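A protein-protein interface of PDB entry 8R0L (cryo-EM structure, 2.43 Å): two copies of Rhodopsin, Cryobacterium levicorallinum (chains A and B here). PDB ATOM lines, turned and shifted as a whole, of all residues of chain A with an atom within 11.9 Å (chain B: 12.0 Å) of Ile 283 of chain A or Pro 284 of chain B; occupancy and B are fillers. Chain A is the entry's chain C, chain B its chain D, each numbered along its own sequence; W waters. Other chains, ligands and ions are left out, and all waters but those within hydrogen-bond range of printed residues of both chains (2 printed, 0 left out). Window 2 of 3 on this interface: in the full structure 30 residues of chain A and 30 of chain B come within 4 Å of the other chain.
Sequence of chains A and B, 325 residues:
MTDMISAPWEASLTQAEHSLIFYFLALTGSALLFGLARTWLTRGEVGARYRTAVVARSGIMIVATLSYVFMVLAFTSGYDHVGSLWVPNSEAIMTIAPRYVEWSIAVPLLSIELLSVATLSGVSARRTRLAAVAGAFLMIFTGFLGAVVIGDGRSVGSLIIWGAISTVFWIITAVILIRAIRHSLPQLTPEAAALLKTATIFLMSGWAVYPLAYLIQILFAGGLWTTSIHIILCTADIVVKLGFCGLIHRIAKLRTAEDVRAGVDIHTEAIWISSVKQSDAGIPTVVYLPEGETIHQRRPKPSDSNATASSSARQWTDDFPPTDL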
ATOM      1  N   GLY A  44     -17.982   0.782  37.170  1.00  0.00           N
ATOM      2  CA  GLY A  44     -17.951   0.082  35.911  1.00  0.00           C
ATOM      3  C   GLY A  44     -18.876   0.661  34.861  1.00  0.00           C
ATOM      4  O   GLY A  44     -18.883   0.153  33.750  1.00  0.00           O
ATOM      5  N   ASP A 259     -18.661   6.989  22.633  1.00  0.00           N
ATOM      6  CA  ASP A 259     -17.499   6.272  22.153  1.00  0.00           C
ATOM      7  C   ASP A 259     -17.851   4.859  21.727  1.00  0.00           C
ATOM      8  O   ASP A 259     -17.244   4.348  20.796  1.00  0.00           O
ATOM      9  CB  ASP A 259     -16.421   6.246  23.235  1.00  0.00           C
ATOM     10  CG  ASP A 259     -15.710   7.593  23.398  1.00  0.00           C
ATOM     11  OD1 ASP A 259     -15.740   8.410  22.410  1.00  0.00           O
ATOM     12  OD2 ASP A 259     -15.161   7.861  24.514  1.00  0.00           O
ATOM     13  N   VAL A 260     -18.830   4.247  22.418  1.00  0.00           N
ATOM     14  CA  VAL A 260     -19.303   2.913  22.094  1.00  0.00           C
ATOM     15  C   VAL A 260     -20.072   2.947  20.787  1.00  0.00           C
ATOM     16  O   VAL A 260     -19.843   2.130  19.912  1.00  0.00           O
ATOM     17  CB  VAL A 260     -20.100   2.294  23.234  1.00  0.00           C
ATOM     18  CG1 VAL A 260     -20.947   1.151  22.738  1.00  0.00           C
ATOM     19  CG2 VAL A 260     -19.195   1.837  24.360  1.00  0.00           C
ATOM     20  N   ARG A 261     -20.852   3.976  20.581  1.00  0.00           N
ATOM     21  CA  ARG A 261     -21.598   4.071  19.346  1.00  0.00           C
ATOM     22  C   ARG A 261     -20.698   4.427  18.169  1.00  0.00           C
ATOM     23  O   ARG A 261     -21.026   4.073  17.042  1.00  0.00           O
ATOM     24  CB  ARG A 261     -22.739   5.057  19.558  1.00  0.00           C
ATOM     25  CG  ARG A 261     -23.752   4.544  20.576  1.00  0.00           C
ATOM     26  CD  ARG A 261     -24.998   5.407  20.616  1.00  0.00           C
ATOM     27  NE  ARG A 261     -24.658   6.826  20.686  1.00  0.00           N
ATOM     28  CZ  ARG A 261     -24.756   7.598  21.765  1.00  0.00           C
ATOM     29  NH1 ARG A 261     -25.235   7.134  22.909  1.00  0.00           N
ATOM     30  NH2 ARG A 261     -24.389   8.864  21.676  1.00  0.00           N
ATOM     31  N   GLY A 263     -17.571   3.340  17.844  1.00  0.00           N
ATOM     32  CA  GLY A 263     -16.555   2.326  17.665  1.00  0.00           C
ATOM     33  C   GLY A 263     -15.203   2.701  18.258  1.00  0.00           C
ATOM     34  O   GLY A 263     -14.244   1.941  18.162  1.00  0.00           O
ATOM     35  N   VAL A 264     -15.133   3.845  18.911  1.00  0.00           N
ATOM     36  CA  VAL A 264     -13.908   4.281  19.549  1.00  0.00           C
ATOM     37  C   VAL A 264     -13.521   3.327  20.672  1.00  0.00           C
ATOM     38  O   VAL A 264     -12.342   3.212  20.975  1.00  0.00           O
ATOM     39  CB  VAL A 264     -14.091   5.718  20.045  1.00  0.00           C
ATOM     40  CG1 VAL A 264     -12.992   6.169  20.985  1.00  0.00           C
ATOM     41  CG2 VAL A 264     -14.224   6.635  18.850  1.00  0.00           C
ATOM     42  N   ASP A 265     -14.488   2.659  21.298  1.00  0.00           N
ATOM     43  CA  ASP A 265     -14.180   1.673  22.327  1.00  0.00           C
ATOM     44  C   ASP A 265     -15.377   0.745  22.525  1.00  0.00           C
ATOM     45  O   ASP A 265     -16.389   0.889  21.855  1.00  0.00           O
ATOM     46  CB  ASP A 265     -13.735   2.373  23.611  1.00  0.00           C
ATOM     47  CG  ASP A 265     -12.767   1.605  24.509  1.00  0.00           C
ATOM     48  OD1 ASP A 265     -12.546   0.388  24.275  1.00  0.00           O
ATOM     49  OD2 ASP A 265     -12.256   2.237  25.477  1.00  0.00           O
ATOM     50  N   ILE A 266     -15.223  -0.269  23.369  1.00  0.00           N
ATOM     51  CA  ILE A 266     -16.316  -1.168  23.681  1.00  0.00           C
ATOM     52  C   ILE A 266     -16.544  -1.072  25.184  1.00  0.00           C
ATOM     53  O   ILE A 266     -15.645  -0.716  25.923  1.00  0.00           O
ATOM     54  CB  ILE A 266     -16.054  -2.607  23.186  1.00  0.00           C
ATOM     55  CG1 ILE A 266     -14.884  -3.287  23.885  1.00  0.00           C
ATOM     56  CG2 ILE A 266     -15.827  -2.626  21.696  1.00  0.00           C
ATOM     57  CD1 ILE A 266     -15.305  -4.260  24.945  1.00  0.00           C
ATOM     58  N   HIS A 267     -17.764  -1.344  25.629  1.00  0.00           N
ATOM     59  CA  HIS A 267     -18.039  -1.363  27.049  1.00  0.00           C
ATOM     60  C   HIS A 267     -18.762  -2.660  27.366  1.00  0.00           C
ATOM     61  O   HIS A 267     -19.645  -3.074  26.620  1.00  0.00           O
ATOM     62  CB  HIS A 267     -18.838  -0.120  27.437  1.00  0.00           C
ATOM     63  CG  HIS A 267     -18.740   0.178  28.883  1.00  0.00           C
ATOM     64  ND1 HIS A 267     -19.821   0.073  29.724  1.00  0.00           N
ATOM     65  CD2 HIS A 267     -17.702   0.570  29.641  1.00  0.00           C
ATOM     66  CE1 HIS A 267     -19.423   0.382  30.950  1.00  0.00           C
ATOM     67  NE2 HIS A 267     -18.141   0.692  30.928  1.00  0.00           N
ATOM     68  N   THR A 268     -18.425  -3.275  28.488  1.00  0.00           N
ATOM     69  CA  THR A 268     -18.921  -4.609  28.777  1.00  0.00           C
ATOM     70  C   THR A 268     -20.392  -4.633  29.179  1.00  0.00           C
ATOM     71  O   THR A 268     -21.041  -5.667  29.089  1.00  0.00           O
ATOM     72  CB  THR A 268     -18.073  -5.257  29.866  1.00  0.00           C
ATOM     73  OG1 THR A 268     -17.688  -4.224  30.779  1.00  0.00           O
ATOM     74  CG2 THR A 268     -16.853  -5.915  29.264  1.00  0.00           C
ATOM     75  N   GLU A 269     -20.912  -3.506  29.625  1.00  0.00           N
ATOM     76  CA  GLU A 269     -22.280  -3.420  30.076  1.00  0.00           C
ATOM     77  C   GLU A 269     -22.982  -2.369  29.237  1.00  0.00           C
ATOM     78  O   GLU A 269     -22.310  -1.461  28.734  1.00  0.00           O
ATOM     79  CB  GLU A 269     -22.200  -3.002  31.533  1.00  0.00           C
ATOM     80  CG  GLU A 269     -23.342  -3.491  32.387  1.00  0.00           C
ATOM     81  CD  GLU A 269     -23.043  -3.208  33.859  1.00  0.00           C
ATOM     82  OE1 GLU A 269     -23.407  -4.081  34.728  1.00  0.00           O
ATOM     83  OE2 GLU A 269     -22.410  -2.125  34.138  1.00  0.00           O
ATOM     84  N   ALA A 270     -24.318  -2.447  29.172  1.00  0.00           N
ATOM     85  CA  ALA A 270     -25.099  -1.345  28.631  1.00  0.00           C
ATOM     86  C   ALA A 270     -25.031  -0.135  29.562  1.00  0.00           C
ATOM     87  O   ALA A 270     -24.842  -0.308  30.760  1.00  0.00           O
ATOM     88  CB  ALA A 270     -26.504  -1.747  28.392  1.00  0.00           C
ATOM     89  N   ILE A 271     -25.112   1.073  28.982  1.00  0.00           N
ATOM     90  CA  ILE A 271     -25.157   2.281  29.770  1.00  0.00           C
ATOM     91  C   ILE A 271     -26.585   2.792  29.775  1.00  0.00           C
ATOM     92  O   ILE A 271     -27.223   2.911  28.734  1.00  0.00           O
ATOM     93  CB  ILE A 271     -24.123   3.315  29.275  1.00  0.00           C
ATOM     94  CG1 ILE A 271     -22.716   2.880  29.690  1.00  0.00           C
ATOM     95  CG2 ILE A 271     -24.417   4.724  29.800  1.00  0.00           C
ATOM     96  CD1 ILE A 271     -21.700   3.019  28.640  1.00  0.00           C
ATOM     97  N   LYS A 277     -31.545   3.807  27.583  1.00  0.00           N
ATOM     98  CA  LYS A 277     -30.339   3.094  27.216  1.00  0.00           C
ATOM     99  C   LYS A 277     -29.548   3.984  26.277  1.00  0.00           C
ATOM    100  O   LYS A 277     -30.094   4.466  25.292  1.00  0.00           O
ATOM    101  CB  LYS A 277     -30.671   1.772  26.523  1.00  0.00           C
ATOM    102  CG  LYS A 277     -29.627   0.694  26.675  1.00  0.00           C
ATOM    103  CD  LYS A 277     -29.728  -0.347  25.640  1.00  0.00           C
ATOM    104  CE  LYS A 277     -29.437  -1.720  26.204  1.00  0.00           C
ATOM    105  NZ  LYS A 277     -28.988  -2.675  25.155  1.00  0.00           N
ATOM    106  N   SER A 279     -26.244   2.908  25.250  1.00  0.00           N
ATOM    107  CA  SER A 279     -25.334   2.064  24.501  1.00  0.00           C
ATOM    108  C   SER A 279     -25.552   0.638  24.960  1.00  0.00           C
ATOM    109  O   SER A 279     -25.936   0.432  26.094  1.00  0.00           O
ATOM    110  CB  SER A 279     -23.866   2.493  24.628  1.00  0.00           C
ATOM    111  OG  SER A 279     -23.293   2.144  25.893  1.00  0.00           O
ATOM    112  N   ASP A 280     -25.242  -0.326  24.081  1.00  0.00           N
ATOM    113  CA  ASP A 280     -25.387  -1.737  24.390  1.00  0.00           C
ATOM    114  C   ASP A 280     -24.082  -2.318  24.883  1.00  0.00           C
ATOM    115  O   ASP A 280     -23.027  -1.726  24.675  1.00  0.00           O
ATOM    116  CB  ASP A 280     -25.843  -2.520  23.175  1.00  0.00           C
ATOM    117  CG  ASP A 280     -27.106  -1.938  22.557  1.00  0.00           C
ATOM    118  OD1 ASP A 280     -27.445  -0.771  22.893  1.00  0.00           O
ATOM    119  OD2 ASP A 280     -27.756  -2.654  21.754  1.00  0.00           O
ATOM    120  N   ALA A 281     -24.188  -3.468  25.555  1.00  0.00           N
ATOM    121  CA  ALA A 281     -23.039  -4.265  25.943  1.00  0.00           C
ATOM    122  C   ALA A 281     -22.369  -4.829  24.694  1.00  0.00           C
ATOM    123  O   ALA A 281     -23.051  -5.170  23.727  1.00  0.00           O
ATOM    124  CB  ALA A 281     -23.480  -5.370  26.855  1.00  0.00           C
ATOM    125  N   GLY A 282     -21.037  -4.896  24.719  1.00  0.00           N
ATOM    126  CA  GLY A 282     -20.293  -5.468  23.616  1.00  0.00           C
ATOM    127  C   GLY A 282     -19.108  -6.295  24.107  1.00  0.00           C
ATOM    128  O   GLY A 282     -18.778  -6.267  25.294  1.00  0.00           O
ATOM    129  N   ILE A 283     -18.476  -7.032  23.180  1.00  0.00           N
ATOM    130  CA  ILE A 283     -17.389  -7.942  23.521  1.00  0.00           C
ATOM    131  C   ILE A 283     -16.136  -7.541  22.750  1.00  0.00           C
ATOM    132  O   ILE A 283     -16.211  -7.251  21.554  1.00  0.00           O
ATOM    133  CB  ILE A 283     -17.755  -9.419  23.256  1.00  0.00           C
ATOM    134  CG1 ILE A 283     -18.818  -9.545  22.156  1.00  0.00           C
ATOM    135  CG2 ILE A 283     -18.175 -10.108  24.550  1.00  0.00           C
ATOM    136  CD1 ILE A 283     -19.121 -10.964  21.720  1.00  0.00           C
ATOM    137  N   PRO A 284     -14.961  -7.520  23.432  1.00  0.00           N
ATOM    138  CA  PRO A 284     -13.672  -7.205  22.804  1.00  0.00           C
ATOM    139  C   PRO A 284     -13.492  -7.731  21.372  1.00  0.00           C
ATOM    140  O   PRO A 284     -14.079  -8.761  21.075  1.00  0.00           O
ATOM    141  CB  PRO A 284     -12.702  -7.904  23.763  1.00  0.00           C
ATOM    142  CG  PRO A 284     -13.327  -7.672  25.130  1.00  0.00           C
ATOM    143  CD  PRO A 284     -14.821  -7.771  24.881  1.00  0.00           C
ATOM    144  N   ALA B  48     -27.858  -3.131  35.157  1.00  0.00           N
ATOM    145  CA  ALA B  48     -27.450  -1.753  35.259  1.00  0.00           C
ATOM    146  C   ALA B  48     -28.636  -0.787  35.134  1.00  0.00           C
ATOM    147  O   ALA B  48     -28.514   0.328  35.627  1.00  0.00           O
ATOM    148  CB  ALA B  48     -26.408  -1.530  34.177  1.00  0.00           C
ATOM    149  N   VAL B 260     -34.224  -9.209  29.977  1.00  0.00           N
ATOM    150  CA  VAL B 260     -33.400 -10.220  29.337  1.00  0.00           C
ATOM    151  C   VAL B 260     -34.249 -11.054  28.393  1.00  0.00           C
ATOM    152  O   VAL B 260     -33.870 -11.277  27.257  1.00  0.00           O
ATOM    153  CB  VAL B 260     -32.638 -11.060  30.352  1.00  0.00           C
ATOM    154  CG1 VAL B 260     -32.173 -12.353  29.735  1.00  0.00           C
ATOM    155  CG2 VAL B 260     -31.469 -10.298  30.942  1.00  0.00           C
ATOM    156  N   GLY B 263     -35.065  -8.959  25.227  1.00  0.00           N
ATOM    157  CA  GLY B 263     -33.965  -8.471  24.426  1.00  0.00           C
ATOM    158  C   GLY B 263     -33.585  -7.027  24.723  1.00  0.00           C
ATOM    159  O   GLY B 263     -32.679  -6.479  24.101  1.00  0.00           O
ATOM    160  N   VAL B 264     -34.239  -6.421  25.696  1.00  0.00           N
ATOM    161  CA  VAL B 264     -33.929  -5.060  26.086  1.00  0.00           C
ATOM    162  C   VAL B 264     -32.509  -4.970  26.633  1.00  0.00           C
ATOM    163  O   VAL B 264     -31.895  -3.916  26.532  1.00  0.00           O
ATOM    164  CB  VAL B 264     -34.967  -4.584  27.104  1.00  0.00           C
ATOM    165  CG1 VAL B 264     -34.583  -3.292  27.789  1.00  0.00           C
ATOM    166  CG2 VAL B 264     -36.316  -4.489  26.434  1.00  0.00           C
ATOM    167  N   ASP B 265     -31.989  -6.045  27.224  1.00  0.00           N
ATOM    168  CA  ASP B 265     -30.613  -6.049  27.704  1.00  0.00           C
ATOM    169  C   ASP B 265     -30.133  -7.489  27.880  1.00  0.00           C
ATOM    170  O   ASP B 265     -30.868  -8.424  27.607  1.00  0.00           O
ATOM    171  CB  ASP B 265     -30.494  -5.208  28.975  1.00  0.00           C
ATOM    172  CG  ASP B 265     -29.144  -4.547  29.239  1.00  0.00           C
ATOM    173  OD1 ASP B 265     -28.154  -4.868  28.528  1.00  0.00           O
ATOM    174  OD2 ASP B 265     -29.082  -3.729  30.199  1.00  0.00           O
ATOM    175  N   ILE B 266     -28.866  -7.664  28.231  1.00  0.00           N
ATOM    176  CA  ILE B 266     -28.319  -8.982  28.484  1.00  0.00           C
ATOM    177  C   ILE B 266     -27.814  -8.979  29.921  1.00  0.00           C
ATOM    178  O   ILE B 266     -27.506  -7.935  30.465  1.00  0.00           O
ATOM    179  CB  ILE B 266     -27.239  -9.375  27.452  1.00  0.00           C
ATOM    180  CG1 ILE B 266     -25.999  -8.492  27.507  1.00  0.00           C
ATOM    181  CG2 ILE B 266     -27.806  -9.361  26.053  1.00  0.00           C
ATOM    182  CD1 ILE B 266     -24.843  -9.137  28.195  1.00  0.00           C
ATOM    183  N   HIS B 267     -27.775 -10.144  30.552  1.00  0.00           N
ATOM    184  CA  HIS B 267     -27.241 -10.238  31.894  1.00  0.00           C
ATOM    185  C   HIS B 267     -26.248 -11.388  31.917  1.00  0.00           C
ATOM    186  O   HIS B 267     -26.504 -12.440  31.342  1.00  0.00           O
ATOM    187  CB  HIS B 267     -28.378 -10.415  32.902  1.00  0.00           C
ATOM    188  CG  HIS B 267     -27.971 -10.041  34.275  1.00  0.00           C
ATOM    189  ND1 HIS B 267     -27.864 -10.967  35.286  1.00  0.00           N
ATOM    190  CD2 HIS B 267     -27.638  -8.852  34.809  1.00  0.00           C
ATOM    191  CE1 HIS B 267     -27.464 -10.339  36.384  1.00  0.00           C
ATOM    192  NE2 HIS B 267     -27.323  -9.052  36.122  1.00  0.00           N
ATOM    193  N   THR B 268     -25.136 -11.208  32.611  1.00  0.00           N
ATOM    194  CA  THR B 268     -24.053 -12.173  32.528  1.00  0.00           C
ATOM    195  C   THR B 268     -24.326 -13.463  33.288  1.00  0.00           C
ATOM    196  O   THR B 268     -23.700 -14.482  33.016  1.00  0.00           O
ATOM    197  CB  THR B 268     -22.754 -11.545  33.021  1.00  0.00           C
ATOM    198  OG1 THR B 268     -23.092 -10.653  34.088  1.00  0.00           O
ATOM    199  CG2 THR B 268     -22.069 -10.816  31.887  1.00  0.00           C
ATOM    200  N   GLU B 269     -25.243 -13.423  34.233  1.00  0.00           N
ATOM    201  CA  GLU B 269     -25.555 -14.580  35.040  1.00  0.00           C
ATOM    202  C   GLU B 269     -27.029 -14.888  34.853  1.00  0.00           C
ATOM    203  O   GLU B 269     -27.795 -13.964  34.539  1.00  0.00           O
ATOM    204  CB  GLU B 269     -25.253 -14.174  36.471  1.00  0.00           C
ATOM    205  CG  GLU B 269     -24.813 -15.307  37.362  1.00  0.00           C
ATOM    206  CD  GLU B 269     -24.319 -14.750  38.699  1.00  0.00           C
ATOM    207  OE1 GLU B 269     -23.340 -15.345  39.272  1.00  0.00           O
ATOM    208  OE2 GLU B 269     -24.902 -13.701  39.162  1.00  0.00           O
ATOM    209  N   ALA B 270     -27.421 -16.141  35.131  1.00  0.00           N
ATOM    210  CA  ALA B 270     -28.835 -16.459  35.249  1.00  0.00           C
ATOM    211  C   ALA B 270     -29.426 -15.792  36.491  1.00  0.00           C
ATOM    212  O   ALA B 270     -28.700 -15.554  37.451  1.00  0.00           O
ATOM    213  CB  ALA B 270     -29.059 -17.922  35.277  1.00  0.00           C
ATOM    214  N   ASP B 280     -31.711 -16.685  31.582  1.00  0.00           N
ATOM    215  CA  ASP B 280     -30.437 -17.355  31.396  1.00  0.00           C
ATOM    216  C   ASP B 280     -29.314 -16.350  31.273  1.00  0.00           C
ATOM    217  O   ASP B 280     -29.562 -15.178  31.008  1.00  0.00           O
ATOM    218  CB  ASP B 280     -30.450 -18.228  30.156  1.00  0.00           C
ATOM    219  CG  ASP B 280     -31.613 -19.208  30.158  1.00  0.00           C
ATOM    220  OD1 ASP B 280     -32.560 -19.001  30.967  1.00  0.00           O
ATOM    221  OD2 ASP B 280     -31.571 -20.179  29.362  1.00  0.00           O
ATOM    222  N   ALA B 281     -28.090 -16.837  31.494  1.00  0.00           N
ATOM    223  CA  ALA B 281     -26.879 -16.077  31.244  1.00  0.00           C
ATOM    224  C   ALA B 281     -26.726 -15.841  29.744  1.00  0.00           C
ATOM    225  O   ALA B 281     -27.081 -16.711  28.945  1.00  0.00           O
ATOM    226  CB  ALA B 281     -25.699 -16.825  31.787  1.00  0.00           C
ATOM    227  N   GLY B 282     -26.230 -14.659  29.376  1.00  0.00           N
ATOM    228  CA  GLY B 282     -25.979 -14.356  27.982  1.00  0.00           C
ATOM    229  C   GLY B 282     -24.705 -13.538  27.801  1.00  0.00           C
ATOM    230  O   GLY B 282     -24.122 -13.067  28.774  1.00  0.00           O
ATOM    231  N   ILE B 283     -24.277 -13.373  26.541  1.00  0.00           N
ATOM    232  CA  ILE B 283     -23.033 -12.687  26.213  1.00  0.00           C
ATOM    233  C   ILE B 283     -23.343 -11.514  25.289  1.00  0.00           C
ATOM    234  O   ILE B 283     -24.136 -11.655  24.352  1.00  0.00           O
ATOM    235  CB  ILE B 283     -21.992 -13.640  25.576  1.00  0.00           C
ATOM    236  CG1 ILE B 283     -22.667 -14.813  24.854  1.00  0.00           C
ATOM    237  CG2 ILE B 283     -20.981 -14.103  26.619  1.00  0.00           C
ATOM    238  CD1 ILE B 283     -21.724 -15.704  24.073  1.00  0.00           C
ATOM    239  N   PRO B 284     -22.707 -10.338  25.530  1.00  0.00           N
ATOM    240  CA  PRO B 284     -22.862  -9.150  24.683  1.00  0.00           C
ATOM    241  C   PRO B 284     -22.998  -9.429  23.176  1.00  0.00           C
ATOM    242  O   PRO B 284     -22.431 -10.421  22.734  1.00  0.00           O
ATOM    243  CB  PRO B 284     -21.546  -8.415  24.974  1.00  0.00           C
ATOM    244  CG  PRO B 284     -21.331  -8.657  26.457  1.00  0.00           C
ATOM    245  CD  PRO B 284     -21.801 -10.086  26.668  1.00  0.00           C
HETATM  246  O   HOH W   1     -27.136  -4.506  26.135  1.00  0.00           O
HETATM  247  O   HOH W   2     -26.142  -4.698  30.046  1.00  0.00           O
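No residue of chain B comes within 4 Å of Ile 266 of chain A.
Of the printed residues of chain B, Thr 268 of chain A touches Pro 284 (3.99 Å).
Of the printed residues of chain B, Glu 269 of chain A touches Ala 48 (3.8 Å).
Of the printed residues of chain B, Ala 270 of chain A touches Ala 48 (3.95 Å) and Asp 265 (3.5 Å).
Of the printed residues of chain B, Ala 281 of chain A touches Pro 284.
Printed residues of chain B within 4 Å of Ile 283 of chain A: Pro 284 (3.5 Å).
No residue of chain B comes within 4 Å of Pro 284 of chain A.
Printed residues of chain A within 4 Å of Ala 48 of chain B: Glu 269 and Ala 270.
Of the printed residues of chain A, Val 264 of chain B touches Lys 277.
Thr 268 of chain B touches none of the printed residues of chain A.
Ala 281 of chain B touches none of the printed residues of chain A.
No residue of chain A comes within 4 Å of Gly 282 of chain B.
No residue of chain A comes within 4 Å of Ile 283 of chain B.
Printed residues of chain A within 4 Å of Pro 284 of chain B: Thr 268, Ala 281, Gly 282 and Ile 283.
The nearest printed residue of chain A that does not touch Pro 284 of chain B is His 267 of chain A (5.8 Å).
A ring nitrogen (ND1) of His 267 of chain A is in hydrogen-bond range of the backbone carbonyl oxygen (O) of Glu 269 of chain A, at 3.1 Å.
The backbone NH of Gly 282 of chain A is in hydrogen-bond range of the backbone carbonyl oxygen of His 267 of chain A (3.0 Å).
NZ of Lys 277 of chain A is in salt-bridge range of OD1 of Asp 280 of chain A (3.3 Å).
Printed residues of chain A that touch a printed residue of chain B: Thr 268, Glu 269, Ala 270, Lys 277, Ala 281, Gly 282 and Ile 283.
Hydrophobic or aromatic side chains of chain A within 4 Å of the printed part of chain B: Ala 270, Ala 281 and Ile 283.
Of the 15 printed residues of chain B, 4 touch a printed residue of chain A.
Printed residues of chain B that touch a printed residue of chain A: Ala 48, Val 264, Asp 265 and Pro 284.
Hydrophobic or aromatic side chains of chain B that line the printed part of chain A: Ala 48 and Pro 284.
Among the printed residues, 8 pairs touch across the chains.
Among the printed residues, no Asp or Glu carboxylate lies within 4 Å of a Lys or Arg side-chain nitrogen of the other chain.
Among the printed residues, pairs that only touch across the chains: Gly 282 of chain A with Pro 284 of chain B, Ile 283 of chain A with Pro 284 of chain B, Ala 270 of chain A with Asp 265 of chain B, Ala 281 of chain A with Pro 284 of chain B, Glu 269 of chain A with Ala 48 of chain B, Ala 270 of chain A with Ala 48 of chain B and Thr 268 of chain A with Pro 284 of chain B.
Water W2 lies within hydrogen-bond range of the side-chain carboxylate of Asp 265 of chain B (2.5 Å) and the backbone NH of Ala 270 of chain A (3.0 Å).
Water W1 lies within hydrogen-bond range of OD1 of Asp 265 of chain B (2.6 Å), NZ of Lys 277 of chain A (2.8 Å) and N of Ala 281 of chain A (3.2 Å).
The side-chain amino group (NZ) of Lys 277 of chain A lies close to the backbone carbonyl oxygen (O) of Val 264 of chain B.
Ala 270 of chain A touches Asp 265 of chain B, but with the chains exchanged Asp 265 of chain A does not touch Ala 270 of chain B (24.2 Å).
Ala 281 of chain A touches Pro 284 of chain B, but with the chains exchanged Pro 284 of chain A does not touch Ala 281 of chain B (15.2 Å).
Gly 282 of chain A touches Pro 284 of chain B, but with the chains exchanged Pro 284 of chain A does not touch Gly 282 of chain B (11.4 Å).
Ile 283 of chain A touches Pro 284 of chain B, but with the chains exchanged Pro 284 of chain A does not touch Ile 283 of chain B (9.0 Å).
Positions printed for both chains: 260, 263, 264, 265, 266, 267, 268, 269, 270, 280, 281, 282, 283 and 284.
Of the 8 pairs that touch across the chains among the printed residues, none has its exchanged pair printed and touching as well.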
